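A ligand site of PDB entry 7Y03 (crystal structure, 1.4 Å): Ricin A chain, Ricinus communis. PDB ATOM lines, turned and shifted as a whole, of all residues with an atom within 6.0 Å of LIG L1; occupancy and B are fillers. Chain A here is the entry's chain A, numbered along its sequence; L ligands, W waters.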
ATOM      1  N   ASN A  85       7.238 -19.812  31.656  1.00  0.00           N
ATOM      2  CA  ASN A  85       5.859 -20.191  31.315  1.00  0.00           C
ATOM      3  C   ASN A  85       5.615 -21.701  31.221  1.00  0.00           C
ATOM      4  O   ASN A  85       4.496 -22.114  30.907  1.00  0.00           O
ATOM      5  CB  ASN A  85       5.427 -19.494  30.008  1.00  0.00           C
ATOM      6  CG  ASN A  85       6.406 -19.716  28.869  1.00  0.00           C
ATOM      7  OD1 ASN A  85       7.296 -20.568  28.945  1.00  0.00           O
ATOM      8  ND2 ASN A  85       6.231 -18.962  27.787  1.00  0.00           N
ATOM      9  N   ALA A  86       6.639 -22.505  31.517  1.00  0.00           N
ATOM     10  CA  ALA A  86       6.634 -23.976  31.353  1.00  0.00           C
ATOM     11  C   ALA A  86       6.411 -24.438  29.903  1.00  0.00           C
ATOM     12  O   ALA A  86       6.097 -25.593  29.666  1.00  0.00           O
ATOM     13  CB  ALA A  86       5.635 -24.642  32.313  1.00  0.00           C
ATOM     14  N   TYR A  87       6.611 -23.530  28.944  1.00  0.00           N
ATOM     15  CA  TYR A  87       6.371 -23.824  27.529  1.00  0.00           C
ATOM     16  C   TYR A  87       7.393 -24.824  27.005  1.00  0.00           C
ATOM     17  O   TYR A  87       8.601 -24.663  27.225  1.00  0.00           O
ATOM     18  CB  TYR A  87       6.457 -22.528  26.721  1.00  0.00           C
ATOM     19  CG  TYR A  87       5.898 -22.586  25.329  1.00  0.00           C
ATOM     20  CD1 TYR A  87       6.705 -22.962  24.248  1.00  0.00           C
ATOM     21  CD2 TYR A  87       4.574 -22.220  25.066  1.00  0.00           C
ATOM     22  CE1 TYR A  87       6.195 -23.001  22.953  1.00  0.00           C
ATOM     23  CE2 TYR A  87       4.051 -22.247  23.785  1.00  0.00           C
ATOM     24  CZ  TYR A  87       4.871 -22.642  22.734  1.00  0.00           C
ATOM     25  OH  TYR A  87       4.378 -22.676  21.452  1.00  0.00           O
ATOM     26  N   VAL A  88       6.907 -25.864  26.339  1.00  0.00           N
ATOM     27  CA  VAL A  88       7.765 -26.872  25.726  1.00  0.00           C
ATOM     28  C   VAL A  88       8.272 -26.276  24.403  1.00  0.00           C
ATOM     29  O   VAL A  88       7.492 -26.116  23.450  1.00  0.00           O
ATOM     30  CB  VAL A  88       7.030 -28.214  25.497  1.00  0.00           C
ATOM     31  CG1 VAL A  88       7.957 -29.235  24.856  1.00  0.00           C
ATOM     32  CG2 VAL A  88       6.486 -28.766  26.816  1.00  0.00           C
ATOM     33  N   VAL A  89       9.560 -25.935  24.361  1.00  0.00           N
ATOM     34  CA  VAL A  89      10.148 -25.265  23.189  1.00  0.00           C
ATOM     35  C   VAL A  89      10.675 -26.237  22.138  1.00  0.00           C
ATOM     36  O   VAL A  89      10.865 -25.870  20.978  1.00  0.00           O
ATOM     37  CB  VAL A  89      11.253 -24.246  23.573  1.00  0.00           C
ATOM     38  CG1 VAL A  89      10.703 -23.141  24.467  1.00  0.00           C
ATOM     39  CG2 VAL A  89      12.453 -24.912  24.232  1.00  0.00           C
ATOM     40  N   PHE A 100      10.227 -25.921  18.037  1.00  0.00           N
ATOM     41  CA  PHE A 100       9.116 -25.206  17.409  1.00  0.00           C
ATOM     42  C   PHE A 100       9.592 -23.871  16.866  1.00  0.00           C
ATOM     43  O   PHE A 100      10.569 -23.304  17.379  1.00  0.00           O
ATOM     44  CB  PHE A 100       7.968 -24.997  18.397  1.00  0.00           C
ATOM     45  CG  PHE A 100       7.352 -26.277  18.896  1.00  0.00           C
ATOM     46  CD1 PHE A 100       6.676 -27.134  18.014  1.00  0.00           C
ATOM     47  CD2 PHE A 100       7.448 -26.639  20.236  1.00  0.00           C
ATOM     48  CE1 PHE A 100       6.108 -28.317  18.473  1.00  0.00           C
ATOM     49  CE2 PHE A 100       6.880 -27.822  20.695  1.00  0.00           C
ATOM     50  CZ  PHE A 100       6.216 -28.657  19.812  1.00  0.00           C
ATOM     51  N   GLY A 128       4.454 -23.888  18.214  1.00  0.00           N
ATOM     52  CA  GLY A 128       4.062 -24.966  19.112  1.00  0.00           C
ATOM     53  C   GLY A 128       2.806 -24.787  19.948  1.00  0.00           C
ATOM     54  O   GLY A 128       2.577 -25.592  20.849  1.00  0.00           O
ATOM     55  N   ASN A 129       2.001 -23.764  19.669  1.00  0.00           N
ATOM     56  CA  ASN A 129       0.743 -23.547  20.400  1.00  0.00           C
ATOM     57  C   ASN A 129      -0.290 -24.616  20.042  1.00  0.00           C
ATOM     58  O   ASN A 129      -0.211 -25.209  18.957  1.00  0.00           O
ATOM     59  CB  ASN A 129       0.162 -22.153  20.123  1.00  0.00           C
ATOM     60  CG  ASN A 129       1.013 -21.030  20.684  1.00  0.00           C
ATOM     61  OD1 ASN A 129       2.029 -21.233  21.347  1.00  0.00           O
ATOM     62  ND2 ASN A 129       0.588 -19.797  20.396  1.00  0.00           N
ATOM     63  N   TYR A 130      -1.243 -24.853  20.951  1.00  0.00           N
ATOM     64  CA  TYR A 130      -2.278 -25.872  20.733  1.00  0.00           C
ATOM     65  C   TYR A 130      -3.002 -25.733  19.400  1.00  0.00           C
ATOM     66  O   TYR A 130      -3.199 -26.728  18.707  1.00  0.00           O
ATOM     67  CB  TYR A 130      -3.322 -25.909  21.853  1.00  0.00           C
ATOM     68  CG  TYR A 130      -2.846 -26.428  23.198  1.00  0.00           C
ATOM     69  CD1 TYR A 130      -2.027 -27.562  23.310  1.00  0.00           C
ATOM     70  CD2 TYR A 130      -3.276 -25.807  24.371  1.00  0.00           C
ATOM     71  CE1 TYR A 130      -1.625 -28.034  24.553  1.00  0.00           C
ATOM     72  CE2 TYR A 130      -2.871 -26.257  25.611  1.00  0.00           C
ATOM     73  CZ  TYR A 130      -2.054 -27.373  25.695  1.00  0.00           C
ATOM     74  OH  TYR A 130      -1.678 -27.806  26.930  1.00  0.00           O
ATOM     75  N   ASP A 131      -3.390 -24.505  19.047  1.00  0.00           N
ATOM     76  CA  ASP A 131      -4.164 -24.272  17.811  1.00  0.00           C
ATOM     77  C   ASP A 131      -3.436 -24.789  16.554  1.00  0.00           C
ATOM     78  O   ASP A 131      -4.046 -25.487  15.743  1.00  0.00           O
ATOM     79  CB  ASP A 131      -4.628 -22.815  17.663  1.00  0.00           C
ATOM     80  CG  ASP A 131      -3.495 -21.779  17.658  1.00  0.00           C
ATOM     81  OD1 ASP A 131      -2.298 -22.125  17.816  1.00  0.00           O
ATOM     82  OD2 ASP A 131      -3.810 -20.584  17.497  1.00  0.00           O
ATOM     83  N   LEU A 133      -0.910 -27.043  16.626  1.00  0.00           N
ATOM     84  CA  LEU A 133      -0.689 -28.481  16.800  1.00  0.00           C
ATOM     85  C   LEU A 133      -1.934 -29.305  16.532  1.00  0.00           C
ATOM     86  O   LEU A 133      -1.846 -30.393  15.953  1.00  0.00           O
ATOM     87  CB  LEU A 133      -0.116 -28.788  18.193  1.00  0.00           C
ATOM     88  CG  LEU A 133       1.317 -28.315  18.512  1.00  0.00           C
ATOM     89  CD1 LEU A 133       1.626 -28.671  19.954  1.00  0.00           C
ATOM     90  CD2 LEU A 133       2.380 -28.895  17.587  1.00  0.00           C
ATOM     91  N   ARG A 141      -7.857 -31.032  21.182  1.00  0.00           N
ATOM     92  CA  ARG A 141      -7.554 -31.551  22.518  1.00  0.00           C
ATOM     93  C   ARG A 141      -8.707 -32.382  23.101  1.00  0.00           C
ATOM     94  O   ARG A 141      -8.460 -33.428  23.694  1.00  0.00           O
ATOM     95  CB  ARG A 141      -7.195 -30.415  23.467  1.00  0.00           C
ATOM     96  CG  ARG A 141      -5.768 -29.919  23.372  1.00  0.00           C
ATOM     97  CD  ARG A 141      -5.618 -28.638  24.169  1.00  0.00           C
ATOM     98  NE  ARG A 141      -6.218 -27.488  23.489  1.00  0.00           N
ATOM     99  CZ  ARG A 141      -6.651 -26.384  24.089  1.00  0.00           C
ATOM    100  NH1 ARG A 141      -6.565 -26.242  25.411  1.00  0.00           N
ATOM    101  NH2 ARG A 141      -7.169 -25.402  23.363  1.00  0.00           N
ATOM    102  N   ILE A 179       2.574 -32.002  26.446  1.00  0.00           N
ATOM    103  CA  ILE A 179       2.366 -30.651  26.964  1.00  0.00           C
ATOM    104  C   ILE A 179       1.347 -30.678  28.108  1.00  0.00           C
ATOM    105  O   ILE A 179       1.569 -30.062  29.158  1.00  0.00           O
ATOM    106  CB  ILE A 179       1.938 -29.668  25.848  1.00  0.00           C
ATOM    107  CG1 ILE A 179       3.087 -29.453  24.856  1.00  0.00           C
ATOM    108  CG2 ILE A 179       1.505 -28.340  26.429  1.00  0.00           C
ATOM    109  CD1 ILE A 179       2.645 -28.989  23.483  1.00  0.00           C
ATOM    110  N   SER A 183       3.423 -29.913  31.338  1.00  0.00           N
ATOM    111  CA  SER A 183       3.305 -28.476  31.568  1.00  0.00           C
ATOM    112  C   SER A 183       1.990 -28.066  32.215  1.00  0.00           C
ATOM    113  O   SER A 183       1.990 -27.324  33.203  1.00  0.00           O
ATOM    114  CB  SER A 183       3.557 -27.685  30.287  1.00  0.00           C
ATOM    115  OG  SER A 183       4.844 -28.001  29.778  1.00  0.00           O
ATOM    116  N   GLU A 184       0.858 -28.554  31.687  1.00  0.00           N
ATOM    117  CA  GLU A 184      -0.437 -28.200  32.280  1.00  0.00           C
ATOM    118  C   GLU A 184      -0.627 -28.767  33.669  1.00  0.00           C
ATOM    119  O   GLU A 184      -1.194 -28.116  34.537  1.00  0.00           O
ATOM    120  CB  GLU A 184      -1.623 -28.585  31.383  1.00  0.00           C
ATOM    121  CG  GLU A 184      -1.624 -27.975  29.987  1.00  0.00           C
ATOM    122  CD  GLU A 184      -1.825 -26.468  29.916  1.00  0.00           C
ATOM    123  OE1 GLU A 184      -1.822 -25.763  30.959  1.00  0.00           O
ATOM    124  OE2 GLU A 184      -1.974 -25.971  28.781  1.00  0.00           O
ATOM    125  N   ARG A 187       1.281 -26.532  35.960  1.00  0.00           N
ATOM    126  CA  ARG A 187       0.572 -25.262  36.149  1.00  0.00           C
ATOM    127  C   ARG A 187      -0.652 -25.396  37.052  1.00  0.00           C
ATOM    128  O   ARG A 187      -0.957 -24.481  37.821  1.00  0.00           O
ATOM    129  CB  ARG A 187       0.132 -24.680  34.801  1.00  0.00           C
ATOM    130  CG  ARG A 187       1.259 -24.233  33.881  1.00  0.00           C
ATOM    131  CD  ARG A 187       0.735 -23.990  32.483  1.00  0.00           C
ATOM    132  NE  ARG A 187       1.823 -23.738  31.539  1.00  0.00           N
ATOM    133  CZ  ARG A 187       1.847 -24.144  30.274  1.00  0.00           C
ATOM    134  NH1 ARG A 187       0.837 -24.861  29.767  1.00  0.00           N
ATOM    135  NH2 ARG A 187       2.890 -23.862  29.514  1.00  0.00           N
ATOM    136  N   GLU A 215      -6.850 -24.768  30.879  1.00  0.00           N
ATOM    137  CA  GLU A 215      -5.729 -24.576  29.950  1.00  0.00           C
ATOM    138  C   GLU A 215      -5.868 -23.277  29.171  1.00  0.00           C
ATOM    139  O   GLU A 215      -4.937 -22.471  29.123  1.00  0.00           O
ATOM    140  CB  GLU A 215      -5.629 -25.746  28.978  1.00  0.00           C
ATOM    141  CG  GLU A 215      -5.319 -27.084  29.641  1.00  0.00           C
ATOM    142  CD  GLU A 215      -5.348 -28.260  28.686  1.00  0.00           C
ATOM    143  OE1 GLU A 215      -5.726 -28.091  27.501  1.00  0.00           O
ATOM    144  OE2 GLU A 215      -5.015 -29.377  29.121  1.00  0.00           O
ATOM    145  N   ASN A 216      -7.051 -23.054  28.600  1.00  0.00           N
ATOM    146  CA  ASN A 216      -7.328 -21.854  27.807  1.00  0.00           C
ATOM    147  C   ASN A 216      -7.322 -20.561  28.603  1.00  0.00           C
ATOM    148  O   ASN A 216      -7.128 -19.484  28.036  1.00  0.00           O
ATOM    149  CB  ASN A 216      -8.661 -22.002  27.068  1.00  0.00           C
ATOM    150  CG  ASN A 216      -8.636 -23.091  26.007  1.00  0.00           C
ATOM    151  OD1 ASN A 216      -7.575 -23.547  25.572  1.00  0.00           O
ATOM    152  ND2 ASN A 216      -9.820 -23.520  25.576  1.00  0.00           N
ATOM    153  N   SER A 217      -7.521 -20.665  29.917  1.00  0.00           N
ATOM    154  CA  SER A 217      -7.649 -19.501  30.799  1.00  0.00           C
ATOM    155  C   SER A 217      -6.434 -19.200  31.677  1.00  0.00           C
ATOM    156  O   SER A 217      -6.495 -18.268  32.470  1.00  0.00           O
ATOM    157  CB  SER A 217      -8.897 -19.623  31.676  1.00  0.00           C
ATOM    158  OG  SER A 217     -10.062 -19.877  30.899  1.00  0.00           O
HETATM  159  N1  LIG L   1      -2.336 -22.552  25.282  1.00  0.00           N
HETATM  160  C1  LIG L   1      -3.492 -21.646  25.010  1.00  0.00           C
HETATM  161  C2  LIG L   1      -4.724 -22.301  24.334  1.00  0.00           C
HETATM  162  O1  LIG L   1      -5.822 -21.810  24.645  1.00  0.00           O
HETATM  163  C3  LIG L   1      -1.549 -23.175  24.373  1.00  0.00           C
HETATM  164  C4  LIG L   1      -3.028 -20.357  24.257  1.00  0.00           C
HETATM  165  C5  LIG L   1      -3.393 -18.603  22.591  1.00  0.00           C
HETATM  166  C6  LIG L   1      -3.816 -19.760  23.262  1.00  0.00           C
HETATM  167  C7  LIG L   1      -2.162 -18.031  22.921  1.00  0.00           C
HETATM  168  C8  LIG L   1      -1.362 -18.607  23.915  1.00  0.00           C
HETATM  169  C9  LIG L   1      -1.802 -19.754  24.576  1.00  0.00           C
HETATM  170  O2  LIG L   1      -4.544 -23.200  23.490  1.00  0.00           O
HETATM  171  O3  LIG L   1      -1.718 -23.067  23.162  1.00  0.00           O
HETATM  172  C10 LIG L   1      -0.388 -23.780  24.876  1.00  0.00           C
HETATM  173  N2  LIG L   1       0.553 -24.231  24.019  1.00  0.00           N
HETATM  174  C11 LIG L   1       1.708 -24.774  24.447  1.00  0.00           C
HETATM  175  N3  LIG L   1       2.598 -25.217  23.548  1.00  0.00           N
HETATM  176  C12 LIG L   1       3.782 -25.743  23.905  1.00  0.00           C
HETATM  177  N4  LIG L   1       4.640 -26.159  22.979  1.00  0.00           N
HETATM  178  N5  LIG L   1       4.109 -25.878  25.258  1.00  0.00           N
HETATM  179  C13 LIG L   1       3.202 -25.438  26.219  1.00  0.00           C
HETATM  180  O4  LIG L   1       3.510 -25.561  27.407  1.00  0.00           O
HETATM  181  C14 LIG L   1       1.982 -24.874  25.813  1.00  0.00           C
HETATM  182  N6  LIG L   1       1.081 -24.445  26.707  1.00  0.00           N
HETATM  183  C15 LIG L   1      -0.125 -23.873  26.248  1.00  0.00           C
HETATM  184  N1  LG2 L   2       3.399 -17.831  25.837  1.00  0.00           N
HETATM  185  C1  LG2 L   2       2.380 -17.373  26.800  1.00  0.00           C
HETATM  186  C2  LG2 L   2       3.060 -16.678  27.984  1.00  0.00           C
HETATM  187  O1  LG2 L   2       2.340 -15.956  28.703  1.00  0.00           O
HETATM  188  C3  LG2 L   2       3.157 -18.207  24.572  1.00  0.00           C
HETATM  189  C4  LG2 L   2       1.565 -18.601  27.283  1.00  0.00           C
HETATM  190  C5  LG2 L   2      -0.536 -19.580  27.969  1.00  0.00           C
HETATM  191  C6  LG2 L   2       0.205 -18.472  27.538  1.00  0.00           C
HETATM  192  C7  LG2 L   2       0.088 -20.821  28.124  1.00  0.00           C
HETATM  193  C8  LG2 L   2       1.456 -20.965  27.870  1.00  0.00           C
HETATM  194  C9  LG2 L   2       2.186 -19.850  27.444  1.00  0.00           C
HETATM  195  O2  LG2 L   2       4.275 -16.868  28.155  1.00  0.00           O
HETATM  196  O3  LG2 L   2       2.044 -18.178  24.036  1.00  0.00           O
HETATM  197  C10 LG2 L   2       4.295 -18.640  23.881  1.00  0.00           C
HETATM  198  N2  LG2 L   2       5.472 -18.789  24.536  1.00  0.00           N
HETATM  199  C11 LG2 L   2       6.595 -19.197  23.911  1.00  0.00           C
HETATM  200  N3  LG2 L   2       7.730 -19.324  24.616  1.00  0.00           N
HETATM  201  C12 LG2 L   2       8.883 -19.732  24.036  1.00  0.00           C
HETATM  202  N4  LG2 L   2       9.999 -19.844  24.739  1.00  0.00           N
HETATM  203  N5  LG2 L   2       8.900 -20.049  22.664  1.00  0.00           N
HETATM  204  C13 LG2 L   2       7.735 -19.935  21.912  1.00  0.00           C
HETATM  205  O4  LG2 L   2       7.772 -20.209  20.714  1.00  0.00           O
HETATM  206  C14 LG2 L   2       6.562 -19.505  22.534  1.00  0.00           C
HETATM  207  N6  LG2 L   2       5.399 -19.374  21.859  1.00  0.00           N
HETATM  208  C15 LG2 L   2       4.231 -18.940  22.505  1.00  0.00           C
HETATM  209  O   HOH W   1      -3.313 -22.122  20.975  1.00  0.00           O
HETATM  210  O   HOH W   2      -6.190 -18.892  25.350  1.00  0.00           O
HETATM  211  O   HOH W   3      -2.164 -19.651  19.750  1.00  0.00           O
HETATM  212  O   HOH W   4      -2.528 -23.341  28.153  1.00  0.00           O
HETATM  213  O   HOH W   5      -6.272 -21.890  21.483  1.00  0.00           O
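The backbone NH (N) of Phe 100 sits at hydrogen-bond distance from the backbone carbonyl oxygen (O) of Val 89 (3.0 Å). The backbone NH (N) of Gly 128 sits close to the side-chain hydroxyl (OH) of Tyr 87 (3.5 Å). The backbone carbonyl oxygen of Ala 86 is in hydrogen-bond range of the side-chain hydroxyl of Ser 183 (2.7 Å). The side-chain hydroxyl of Tyr 130 is in hydrogen-bond range of the side-chain carboxylate of Glu 184, 2.6 Å away. NH2 of Arg 187 sits at hydrogen-bond distance from O of Asn 85 (2.8 Å). The side-chain amide oxygen (OD1) of Asn 216 lies within hydrogen-bond range of the guanidinium group (NH1) of Arg 141, 2.9 Å away. The backbone carbonyl oxygen (O) of Ile 179 lies within hydrogen-bond range of the backbone NH (N) of Glu 184, 3.0 Å away. OH of Tyr 87 lies within hydrogen-bond range of OD1 of Asn 129, at 2.8 Å.
O of Ala 86 sits close to O4 of LIG L1. Merely in contact with LIG L1: Tyr 87 (3.3 Å), Ile 179 (3.4 Å), Ser 183 (3.6 Å), Phe 100 (3.6 Å), Asn 129 (3.7 Å) and Glu 184 (3.8 Å). Hydrophobic or aromatic side chains within 4 Å of LIG L1: Tyr 87, Val 88, Phe 100, Tyr 130 and Ile 179.
O of Gly 128 sits at hydrogen-bond distance from N4 of LIG L1 (3.0 Å). O of Val 88 sits at hydrogen-bond distance from N4 of LIG L1 (2.9 Å). The guanidinium group of Arg 187 lies within hydrogen-bond range of an oxygen (O4) of LIG L1 (2.8 Å). The side-chain amide oxygen (OD1) of Asn 216 sits close to an oxygen (O1) of LIG L1, 2.6 Å away. The backbone NH (N) of Tyr 130 is in hydrogen-bond range of an oxygen (O3) of LIG L1 (2.9 Å). The guanidinium group (NH2) of Arg 141 is in salt-bridge range of an oxygen (O2) of LIG L1, at 3.4 Å. A nitrogen (N6) of LG2 L2 sits close to the side-chain hydroxyl (OH) of Tyr 87. O2 of LG2 L2 is in hydrogen-bond range of ND2 of Asn 85, at 2.9 Å.
Water W1 lies within hydrogen-bond range of an oxygen (O3) of LIG L1 (2.9 Å), the backbone NH (N) of Asp 131 (3.1 Å) and the backbone NH (N) of Tyr 130 (3.4 Å). Water W4 lies within hydrogen-bond range of O of Glu 215, OE2 of Glu 184 and N1 of LIG L1. Water W2 bridges the backbone carbonyl oxygen (O) of Asn 216 and an oxygen (O1) of LIG L1. Water W3 bridges the side-chain amide nitrogen (ND2) of Asn 129 (2.8 Å) and the side-chain carboxylate (OD2) of Asp 131 (2.9 Å).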
